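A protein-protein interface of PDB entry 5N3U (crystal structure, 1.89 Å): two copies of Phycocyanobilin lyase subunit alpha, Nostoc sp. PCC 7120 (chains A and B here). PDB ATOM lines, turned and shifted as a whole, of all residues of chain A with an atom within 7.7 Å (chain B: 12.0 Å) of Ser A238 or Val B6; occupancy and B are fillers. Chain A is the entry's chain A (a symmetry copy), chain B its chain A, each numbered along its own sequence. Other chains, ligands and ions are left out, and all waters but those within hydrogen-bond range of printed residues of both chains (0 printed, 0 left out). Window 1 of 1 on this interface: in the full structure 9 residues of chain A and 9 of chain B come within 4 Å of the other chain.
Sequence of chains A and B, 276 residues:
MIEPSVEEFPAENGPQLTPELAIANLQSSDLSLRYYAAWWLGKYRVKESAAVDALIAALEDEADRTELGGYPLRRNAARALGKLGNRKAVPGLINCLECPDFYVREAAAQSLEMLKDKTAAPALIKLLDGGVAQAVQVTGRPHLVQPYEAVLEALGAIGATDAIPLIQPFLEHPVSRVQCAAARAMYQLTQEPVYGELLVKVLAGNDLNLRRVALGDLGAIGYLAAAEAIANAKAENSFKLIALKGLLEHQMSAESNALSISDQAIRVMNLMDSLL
NZ of Lys A43 is in salt-bridge range of OE1 of Glu B7.
The backbone carbonyl oxygen (O) of Phe B9 is in hydrogen-bond range of the side-chain amino group (NZ) of Lys A43 (2.7 Å).
O of Lys A43 touches CB of Ala B11, at 3.8 Å.
CB of Ser A238 touches CG1 of Val B6, 3.8 Å away.
Phe A239 touches Val B6.
Printed residues of chain B within 4 Å of Lys A43: Glu B7, Phe B9 and Ala B11.
Glu A236 touches none of the printed residues of chain B.
No residue of chain B comes within 4 Å of Asn A237.
Of the printed residues of chain B, Ser A238 touches Val B6 (3.8 Å).
Of chain B, only Val B6 (3.8 Å) comes within 4 Å of Phe A239.
No residue of chain B comes within 4 Å of Leu A241.
Printed residues of chain A within 4 Å of Glu B7: Lys A43.
Of the printed residues of chain A, Phe B9 touches Lys A43.
Printed residues of chain A within 4 Å of Ala B11: Lys A43 (3.8 Å).
The nearest residue of chain A that does not touch Val B6 is Ile A242 (4.1 Å).
Along chain B the printed residues that touch a printed residue of chain A span positions 6 to 11.
Hydrophobic or aromatic side chains of chain A within 4 Å of the printed part of chain B: Phe A239.
Among the printed residues, 5 pairs touch across the chains.
Among the printed residues, Asp or Glu carboxylates within 4 Å of a Lys or Arg side-chain nitrogen of the other chain: Lys A43 with Glu B7 (2.7 Å).
No position is printed for both chains.
Of the 5 pairs that touch across the chains among the printed residues, none has its exchanged pair printed and touching as well.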
ATOM      1  N   LYS A  43      -1.115  19.297 -19.609  1.00  0.00           N
ATOM      2  CA  LYS A  43      -1.478  18.283 -20.553  1.00  0.00           C
ATOM      3  C   LYS A  43      -0.247  17.702 -21.244  1.00  0.00           C
ATOM      4  O   LYS A  43      -0.135  16.506 -21.438  1.00  0.00           O
ATOM      5  CB  LYS A  43      -2.400  18.937 -21.554  1.00  0.00           C
ATOM      6  CG  LYS A  43      -2.745  18.093 -22.792  1.00  0.00           C
ATOM      7  CD  LYS A  43      -3.420  16.794 -22.461  1.00  0.00           C
ATOM      8  CE  LYS A  43      -3.802  16.221 -23.824  1.00  0.00           C
ATOM      9  NZ  LYS A  43      -4.681  15.079 -23.642  1.00  0.00           N
ATOM     10  N   ARG A  45       2.739  17.917 -20.057  1.00  0.00           N
ATOM     11  CA  ARG A  45       3.717  17.466 -19.020  1.00  0.00           C
ATOM     12  C   ARG A  45       5.111  18.145 -19.239  1.00  0.00           C
ATOM     13  O   ARG A  45       6.117  17.492 -19.343  1.00  0.00           O
ATOM     14  CB  ARG A  45       3.841  15.975 -18.977  1.00  0.00           C
ATOM     15  CG  ARG A  45       2.558  15.349 -18.451  1.00  0.00           C
ATOM     16  CD  ARG A  45       2.850  13.997 -17.862  1.00  0.00           C
ATOM     17  NE  ARG A  45       1.578  13.332 -17.607  1.00  0.00           N
ATOM     18  CZ  ARG A  45       1.082  12.996 -16.417  1.00  0.00           C
ATOM     19  NH1 ARG A  45       1.728  13.239 -15.263  1.00  0.00           N
ATOM     20  NH2 ARG A  45      -0.098  12.400 -16.388  1.00  0.00           N
ATOM     21  N   ARG A 212     -14.613   2.971 -12.403  1.00  0.00           N
ATOM     22  CA  ARG A 212     -13.374   3.538 -12.880  1.00  0.00           C
ATOM     23  C   ARG A 212     -12.520   4.007 -11.769  1.00  0.00           C
ATOM     24  O   ARG A 212     -11.313   3.805 -11.738  1.00  0.00           O
ATOM     25  CB  ARG A 212     -13.609   4.686 -13.904  1.00  0.00           C
ATOM     26  CG  ARG A 212     -14.348   4.262 -15.163  1.00  0.00           C
ATOM     27  CD  ARG A 212     -14.653   5.545 -15.928  1.00  0.00           C
ATOM     28  NE  ARG A 212     -15.163   5.320 -17.257  1.00  0.00           N
ATOM     29  CZ  ARG A 212     -15.867   6.224 -17.958  1.00  0.00           C
ATOM     30  NH1 ARG A 212     -16.218   7.380 -17.427  1.00  0.00           N
ATOM     31  NH2 ARG A 212     -16.226   5.965 -19.176  1.00  0.00           N
ATOM     32  N   LEU A 215     -11.007   1.004  -9.996  1.00  0.00           N
ATOM     33  CA  LEU A 215      -9.865   0.557 -10.746  1.00  0.00           C
ATOM     34  C   LEU A 215      -8.632   1.339 -10.474  1.00  0.00           C
ATOM     35  O   LEU A 215      -7.549   0.758 -10.212  1.00  0.00           O
ATOM     36  CB  LEU A 215     -10.171   0.484 -12.249  1.00  0.00           C
ATOM     37  CG  LEU A 215     -11.082  -0.628 -12.585  1.00  0.00           C
ATOM     38  CD1 LEU A 215     -11.748  -0.515 -13.975  1.00  0.00           C
ATOM     39  CD2 LEU A 215     -10.347  -1.954 -12.403  1.00  0.00           C
ATOM     40  N   ALA A 235     -15.675  -2.153 -17.419  1.00  0.00           N
ATOM     41  CA  ALA A 235     -15.098  -0.822 -17.678  1.00  0.00           C
ATOM     42  C   ALA A 235     -14.158  -0.898 -18.836  1.00  0.00           C
ATOM     43  O   ALA A 235     -13.824  -1.996 -19.282  1.00  0.00           O
ATOM     44  CB  ALA A 235     -14.312  -0.375 -16.473  1.00  0.00           C
ATOM     45  N   GLU A 236     -13.653   0.236 -19.261  1.00  0.00           N
ATOM     46  CA  GLU A 236     -12.799   0.246 -20.437  1.00  0.00           C
ATOM     47  C   GLU A 236     -11.451  -0.406 -20.111  1.00  0.00           C
ATOM     48  O   GLU A 236     -10.942  -0.281 -19.007  1.00  0.00           O
ATOM     49  CB  GLU A 236     -12.524   1.684 -20.883  1.00  0.00           C
ATOM     50  CG  GLU A 236     -13.744   2.507 -21.247  1.00  0.00           C
ATOM     51  CD  GLU A 236     -14.682   2.916 -20.052  1.00  0.00           C
ATOM     52  OE1 GLU A 236     -14.326   2.882 -18.849  1.00  0.00           O
ATOM     53  OE2 GLU A 236     -15.832   3.272 -20.339  1.00  0.00           O
ATOM     54  N   ASN A 237     -10.812  -1.029 -21.097  1.00  0.00           N
ATOM     55  CA  ASN A 237      -9.504  -1.654 -20.890  1.00  0.00           C
ATOM     56  C   ASN A 237      -8.457  -0.778 -20.403  1.00  0.00           C
ATOM     57  O   ASN A 237      -7.608  -1.193 -19.645  1.00  0.00           O
ATOM     58  CB  ASN A 237      -9.061  -2.320 -22.198  1.00  0.00           C
ATOM     59  CG  ASN A 237      -9.917  -3.506 -22.535  1.00  0.00           C
ATOM     60  OD1 ASN A 237     -10.597  -4.046 -21.688  1.00  0.00           O
ATOM     61  ND2 ASN A 237      -9.868  -3.920 -23.766  1.00  0.00           N
ATOM     62  N   SER A 238      -8.454   0.481 -20.856  1.00  0.00           N
ATOM     63  CA  SER A 238      -7.522   1.401 -20.335  1.00  0.00           C
ATOM     64  C   SER A 238      -7.447   1.473 -18.834  1.00  0.00           C
ATOM     65  O   SER A 238      -6.370   1.580 -18.267  1.00  0.00           O
ATOM     66  CB  SER A 238      -7.795   2.804 -20.893  1.00  0.00           C
ATOM     67  OG  SER A 238      -7.284   2.846 -22.204  1.00  0.00           O
ATOM     68  N   PHE A 239      -8.583   1.541 -18.186  1.00  0.00           N
ATOM     69  CA  PHE A 239      -8.588   1.560 -16.713  1.00  0.00           C
ATOM     70  C   PHE A 239      -8.163   0.188 -16.148  1.00  0.00           C
ATOM     71  O   PHE A 239      -7.476   0.113 -15.136  1.00  0.00           O
ATOM     72  CB  PHE A 239      -9.969   1.855 -16.219  1.00  0.00           C
ATOM     73  CG  PHE A 239     -10.375   3.246 -16.485  1.00  0.00           C
ATOM     74  CD1 PHE A 239      -9.875   4.272 -15.679  1.00  0.00           C
ATOM     75  CD2 PHE A 239     -11.215   3.543 -17.572  1.00  0.00           C
ATOM     76  CE1 PHE A 239     -10.244   5.640 -15.954  1.00  0.00           C
ATOM     77  CE2 PHE A 239     -11.583   4.877 -17.856  1.00  0.00           C
ATOM     78  CZ  PHE A 239     -11.069   5.916 -17.064  1.00  0.00           C
ATOM     79  N   LYS A 240      -8.609  -0.873 -16.786  1.00  0.00           N
ATOM     80  CA  LYS A 240      -8.149  -2.203 -16.349  1.00  0.00           C
ATOM     81  C   LYS A 240      -6.662  -2.337 -16.389  1.00  0.00           C
ATOM     82  O   LYS A 240      -6.035  -2.854 -15.448  1.00  0.00           O
ATOM     83  CB  LYS A 240      -8.806  -3.301 -17.138  1.00  0.00           C
ATOM     84  CG  LYS A 240     -10.300  -3.328 -16.981  1.00  0.00           C
ATOM     85  CD  LYS A 240     -10.800  -4.549 -17.701  1.00  0.00           C
ATOM     86  CE  LYS A 240     -12.239  -4.528 -17.890  1.00  0.00           C
ATOM     87  NZ  LYS A 240     -12.764  -5.896 -18.169  1.00  0.00           N
ATOM     88  N   LEU A 241      -6.034  -1.845 -17.462  1.00  0.00           N
ATOM     89  CA  LEU A 241      -4.606  -1.974 -17.580  1.00  0.00           C
ATOM     90  C   LEU A 241      -3.865  -1.161 -16.602  1.00  0.00           C
ATOM     91  O   LEU A 241      -2.753  -1.570 -16.122  1.00  0.00           O
ATOM     92  CB  LEU A 241      -4.153  -1.600 -19.035  1.00  0.00           C
ATOM     93  CG  LEU A 241      -4.550  -2.598 -20.106  1.00  0.00           C
ATOM     94  CD1 LEU A 241      -4.420  -1.907 -21.456  1.00  0.00           C
ATOM     95  CD2 LEU A 241      -3.562  -3.781 -19.979  1.00  0.00           C
ATOM     96  N   ILE A 242      -4.401   0.009 -16.282  1.00  0.00           N
ATOM     97  CA  ILE A 242      -3.722   0.826 -15.247  1.00  0.00           C
ATOM     98  C   ILE A 242      -3.797   0.149 -13.882  1.00  0.00           C
ATOM     99  O   ILE A 242      -2.849   0.182 -13.142  1.00  0.00           O
ATOM    100  CB  ILE A 242      -4.369   2.237 -15.109  1.00  0.00           C
ATOM    101  CG1 ILE A 242      -4.113   3.046 -16.336  1.00  0.00           C
ATOM    102  CG2 ILE A 242      -3.812   2.984 -13.900  1.00  0.00           C
ATOM    103  CD1 ILE A 242      -2.644   3.286 -16.542  1.00  0.00           C
ATOM    104  N   ALA A 243      -4.935  -0.438 -13.580  1.00  0.00           N
ATOM    105  CA  ALA A 243      -5.084  -1.162 -12.309  1.00  0.00           C
ATOM    106  C   ALA A 243      -4.129  -2.341 -12.246  1.00  0.00           C
ATOM    107  O   ALA A 243      -3.326  -2.456 -11.308  1.00  0.00           O
ATOM    108  CB  ALA A 243      -6.503  -1.595 -12.191  1.00  0.00           C
ATOM    109  N   LEU A 244      -4.086  -3.132 -13.322  1.00  0.00           N
ATOM    110  CA  LEU A 244      -3.156  -4.286 -13.392  1.00  0.00           C
ATOM    111  C   LEU A 244      -1.741  -3.888 -13.330  1.00  0.00           C
ATOM    112  O   LEU A 244      -0.924  -4.490 -12.661  1.00  0.00           O
ATOM    113  CB  LEU A 244      -3.479  -5.216 -14.589  1.00  0.00           C
ATOM    114  CG  LEU A 244      -4.845  -5.856 -14.510  1.00  0.00           C
ATOM    115  CD1 LEU A 244      -5.355  -6.542 -15.799  1.00  0.00           C
ATOM    116  CD2 LEU A 244      -4.828  -6.893 -13.356  1.00  0.00           C
ATOM    117  N   LEU A 275      -6.231  -8.043 -22.451  1.00  0.00           N
ATOM    118  CA  LEU A 275      -7.039  -6.811 -22.553  1.00  0.00           C
ATOM    119  C   LEU A 275      -6.500  -5.877 -23.660  1.00  0.00           C
ATOM    120  O   LEU A 275      -6.756  -4.657 -23.660  1.00  0.00           O
ATOM    121  CB  LEU A 275      -6.929  -6.122 -21.222  1.00  0.00           C
ATOM    122  CG  LEU A 275      -7.479  -6.934 -20.066  1.00  0.00           C
ATOM    123  CD1 LEU A 275      -7.250  -6.256 -18.742  1.00  0.00           C
ATOM    124  CD2 LEU A 275      -8.963  -7.148 -20.296  1.00  0.00           C
ATOM    125  N   PRO B   4       0.526   8.451 -13.978  1.00  0.00           N
ATOM    126  CA  PRO B   4      -0.265   7.248 -14.424  1.00  0.00           C
ATOM    127  C   PRO B   4      -1.775   7.554 -14.621  1.00  0.00           C
ATOM    128  O   PRO B   4      -2.483   7.667 -13.608  1.00  0.00           O
ATOM    129  CB  PRO B   4      -0.020   6.217 -13.275  1.00  0.00           C
ATOM    130  CG  PRO B   4       0.812   6.969 -12.205  1.00  0.00           C
ATOM    131  CD  PRO B   4       0.801   8.446 -12.530  1.00  0.00           C
ATOM    132  N   SER B   5      -2.261   7.689 -15.870  1.00  0.00           N
ATOM    133  CA  SER B   5      -3.668   8.119 -16.139  1.00  0.00           C
ATOM    134  C   SER B   5      -4.197   7.883 -17.577  1.00  0.00           C
ATOM    135  O   SER B   5      -3.444   7.682 -18.518  1.00  0.00           O
ATOM    136  CB  SER B   5      -3.887   9.608 -15.781  1.00  0.00           C
ATOM    137  OG  SER B   5      -3.730  10.444 -16.921  1.00  0.00           O
ATOM    138  N   VAL B   6      -5.512   7.915 -17.726  1.00  0.00           N
ATOM    139  CA  VAL B   6      -6.134   7.531 -18.944  1.00  0.00           C
ATOM    140  C   VAL B   6      -6.514   8.795 -19.733  1.00  0.00           C
ATOM    141  O   VAL B   6      -7.135   9.687 -19.205  1.00  0.00           O
ATOM    142  CB  VAL B   6      -7.396   6.757 -18.639  1.00  0.00           C
ATOM    143  CG1 VAL B   6      -8.207   6.494 -19.895  1.00  0.00           C
ATOM    144  CG2 VAL B   6      -7.065   5.457 -17.936  1.00  0.00           C
ATOM    145  N   GLU B   7      -6.251   8.813 -21.032  1.00  0.00           N
ATOM    146  CA  GLU B   7      -6.566   9.945 -21.851  1.00  0.00           C
ATOM    147  C   GLU B   7      -7.267   9.443 -23.090  1.00  0.00           C
ATOM    148  O   GLU B   7      -6.805   8.600 -23.843  1.00  0.00           O
ATOM    149  CB  GLU B   7      -5.261  10.661 -22.215  1.00  0.00           C
ATOM    150  CG  GLU B   7      -4.780  11.481 -21.041  1.00  0.00           C
ATOM    151  CD  GLU B   7      -3.484  12.252 -21.341  1.00  0.00           C
ATOM    152  OE1 GLU B   7      -3.502  13.296 -22.055  1.00  0.00           O
ATOM    153  OE2 GLU B   7      -2.447  11.810 -20.833  1.00  0.00           O
ATOM    154  N   GLU B   8      -8.368  10.061 -23.372  1.00  0.00           N
ATOM    155  CA  GLU B   8      -9.047   9.720 -24.580  1.00  0.00           C
ATOM    156  C   GLU B   8      -8.227  10.223 -25.760  1.00  0.00           C
ATOM    157  O   GLU B   8      -8.132   9.563 -26.781  1.00  0.00           O
ATOM    158  CB  GLU B   8     -10.450  10.401 -24.336  1.00  0.00           C
ATOM    159  CG  GLU B   8     -11.408  10.107 -25.289  1.00  0.00           C
ATOM    160  CD  GLU B   8     -12.778  10.743 -25.061  1.00  0.00           C
ATOM    161  OE1 GLU B   8     -12.969  11.849 -24.427  1.00  0.00           O
ATOM    162  OE2 GLU B   8     -13.681  10.080 -25.606  1.00  0.00           O
ATOM    163  N   PHE B   9      -7.664  11.427 -25.689  1.00  0.00           N
ATOM    164  CA  PHE B   9      -6.933  12.010 -26.776  1.00  0.00           C
ATOM    165  C   PHE B   9      -5.490  12.290 -26.238  1.00  0.00           C
ATOM    166  O   PHE B   9      -5.280  13.229 -25.524  1.00  0.00           O
ATOM    167  CB  PHE B   9      -7.515  13.360 -27.181  1.00  0.00           C
ATOM    168  CG  PHE B   9      -9.018  13.381 -27.391  1.00  0.00           C
ATOM    169  CD1 PHE B   9      -9.577  13.036 -28.599  1.00  0.00           C
ATOM    170  CD2 PHE B   9      -9.888  13.887 -26.409  1.00  0.00           C
ATOM    171  CE1 PHE B   9     -10.995  13.153 -28.836  1.00  0.00           C
ATOM    172  CE2 PHE B   9     -11.248  13.914 -26.628  1.00  0.00           C
ATOM    173  CZ  PHE B   9     -11.787  13.567 -27.864  1.00  0.00           C
ATOM    174  N   PRO B  10      -4.571  11.407 -26.485  1.00  0.00           N
ATOM    175  CA  PRO B  10      -3.257  11.584 -25.914  1.00  0.00           C
ATOM    176  C   PRO B  10      -2.441  12.787 -26.418  1.00  0.00           C
ATOM    177  O   PRO B  10      -2.567  13.193 -27.539  1.00  0.00           O
ATOM    178  CB  PRO B  10      -2.596  10.251 -26.228  1.00  0.00           C
ATOM    179  CG  PRO B  10      -3.727   9.286 -26.284  1.00  0.00           C
ATOM    180  CD  PRO B  10      -4.748  10.051 -27.031  1.00  0.00           C
ATOM    181  N   ALA B  11      -1.616  13.359 -25.523  1.00  0.00           N
ATOM    182  CA  ALA B  11      -0.571  14.358 -25.886  1.00  0.00           C
ATOM    183  C   ALA B  11       0.246  13.947 -27.161  1.00  0.00           C
ATOM    184  O   ALA B  11       0.284  14.696 -28.140  1.00  0.00           O
ATOM    185  CB  ALA B  11       0.365  14.592 -24.695  1.00  0.00           C
ATOM    186  N   GLU B  12       0.778  12.712 -27.152  1.00  0.00           N
ATOM    187  CA  GLU B  12       1.544  12.072 -28.296  1.00  0.00           C
ATOM    188  C   GLU B  12       0.830  10.876 -29.024  1.00  0.00           C
ATOM    189  O   GLU B  12       0.069  10.156 -28.405  1.00  0.00           O
ATOM    190  CB  GLU B  12       2.907  11.550 -27.790  1.00  0.00           C
ATOM    191  CG  GLU B  12       2.954  11.042 -26.346  1.00  0.00           C
ATOM    192  CD  GLU B  12       2.017   9.867 -26.031  1.00  0.00           C
ATOM    193  OE1 GLU B  12       2.067   8.831 -26.746  1.00  0.00           O
ATOM    194  OE2 GLU B  12       1.240   9.963 -25.033  1.00  0.00           O
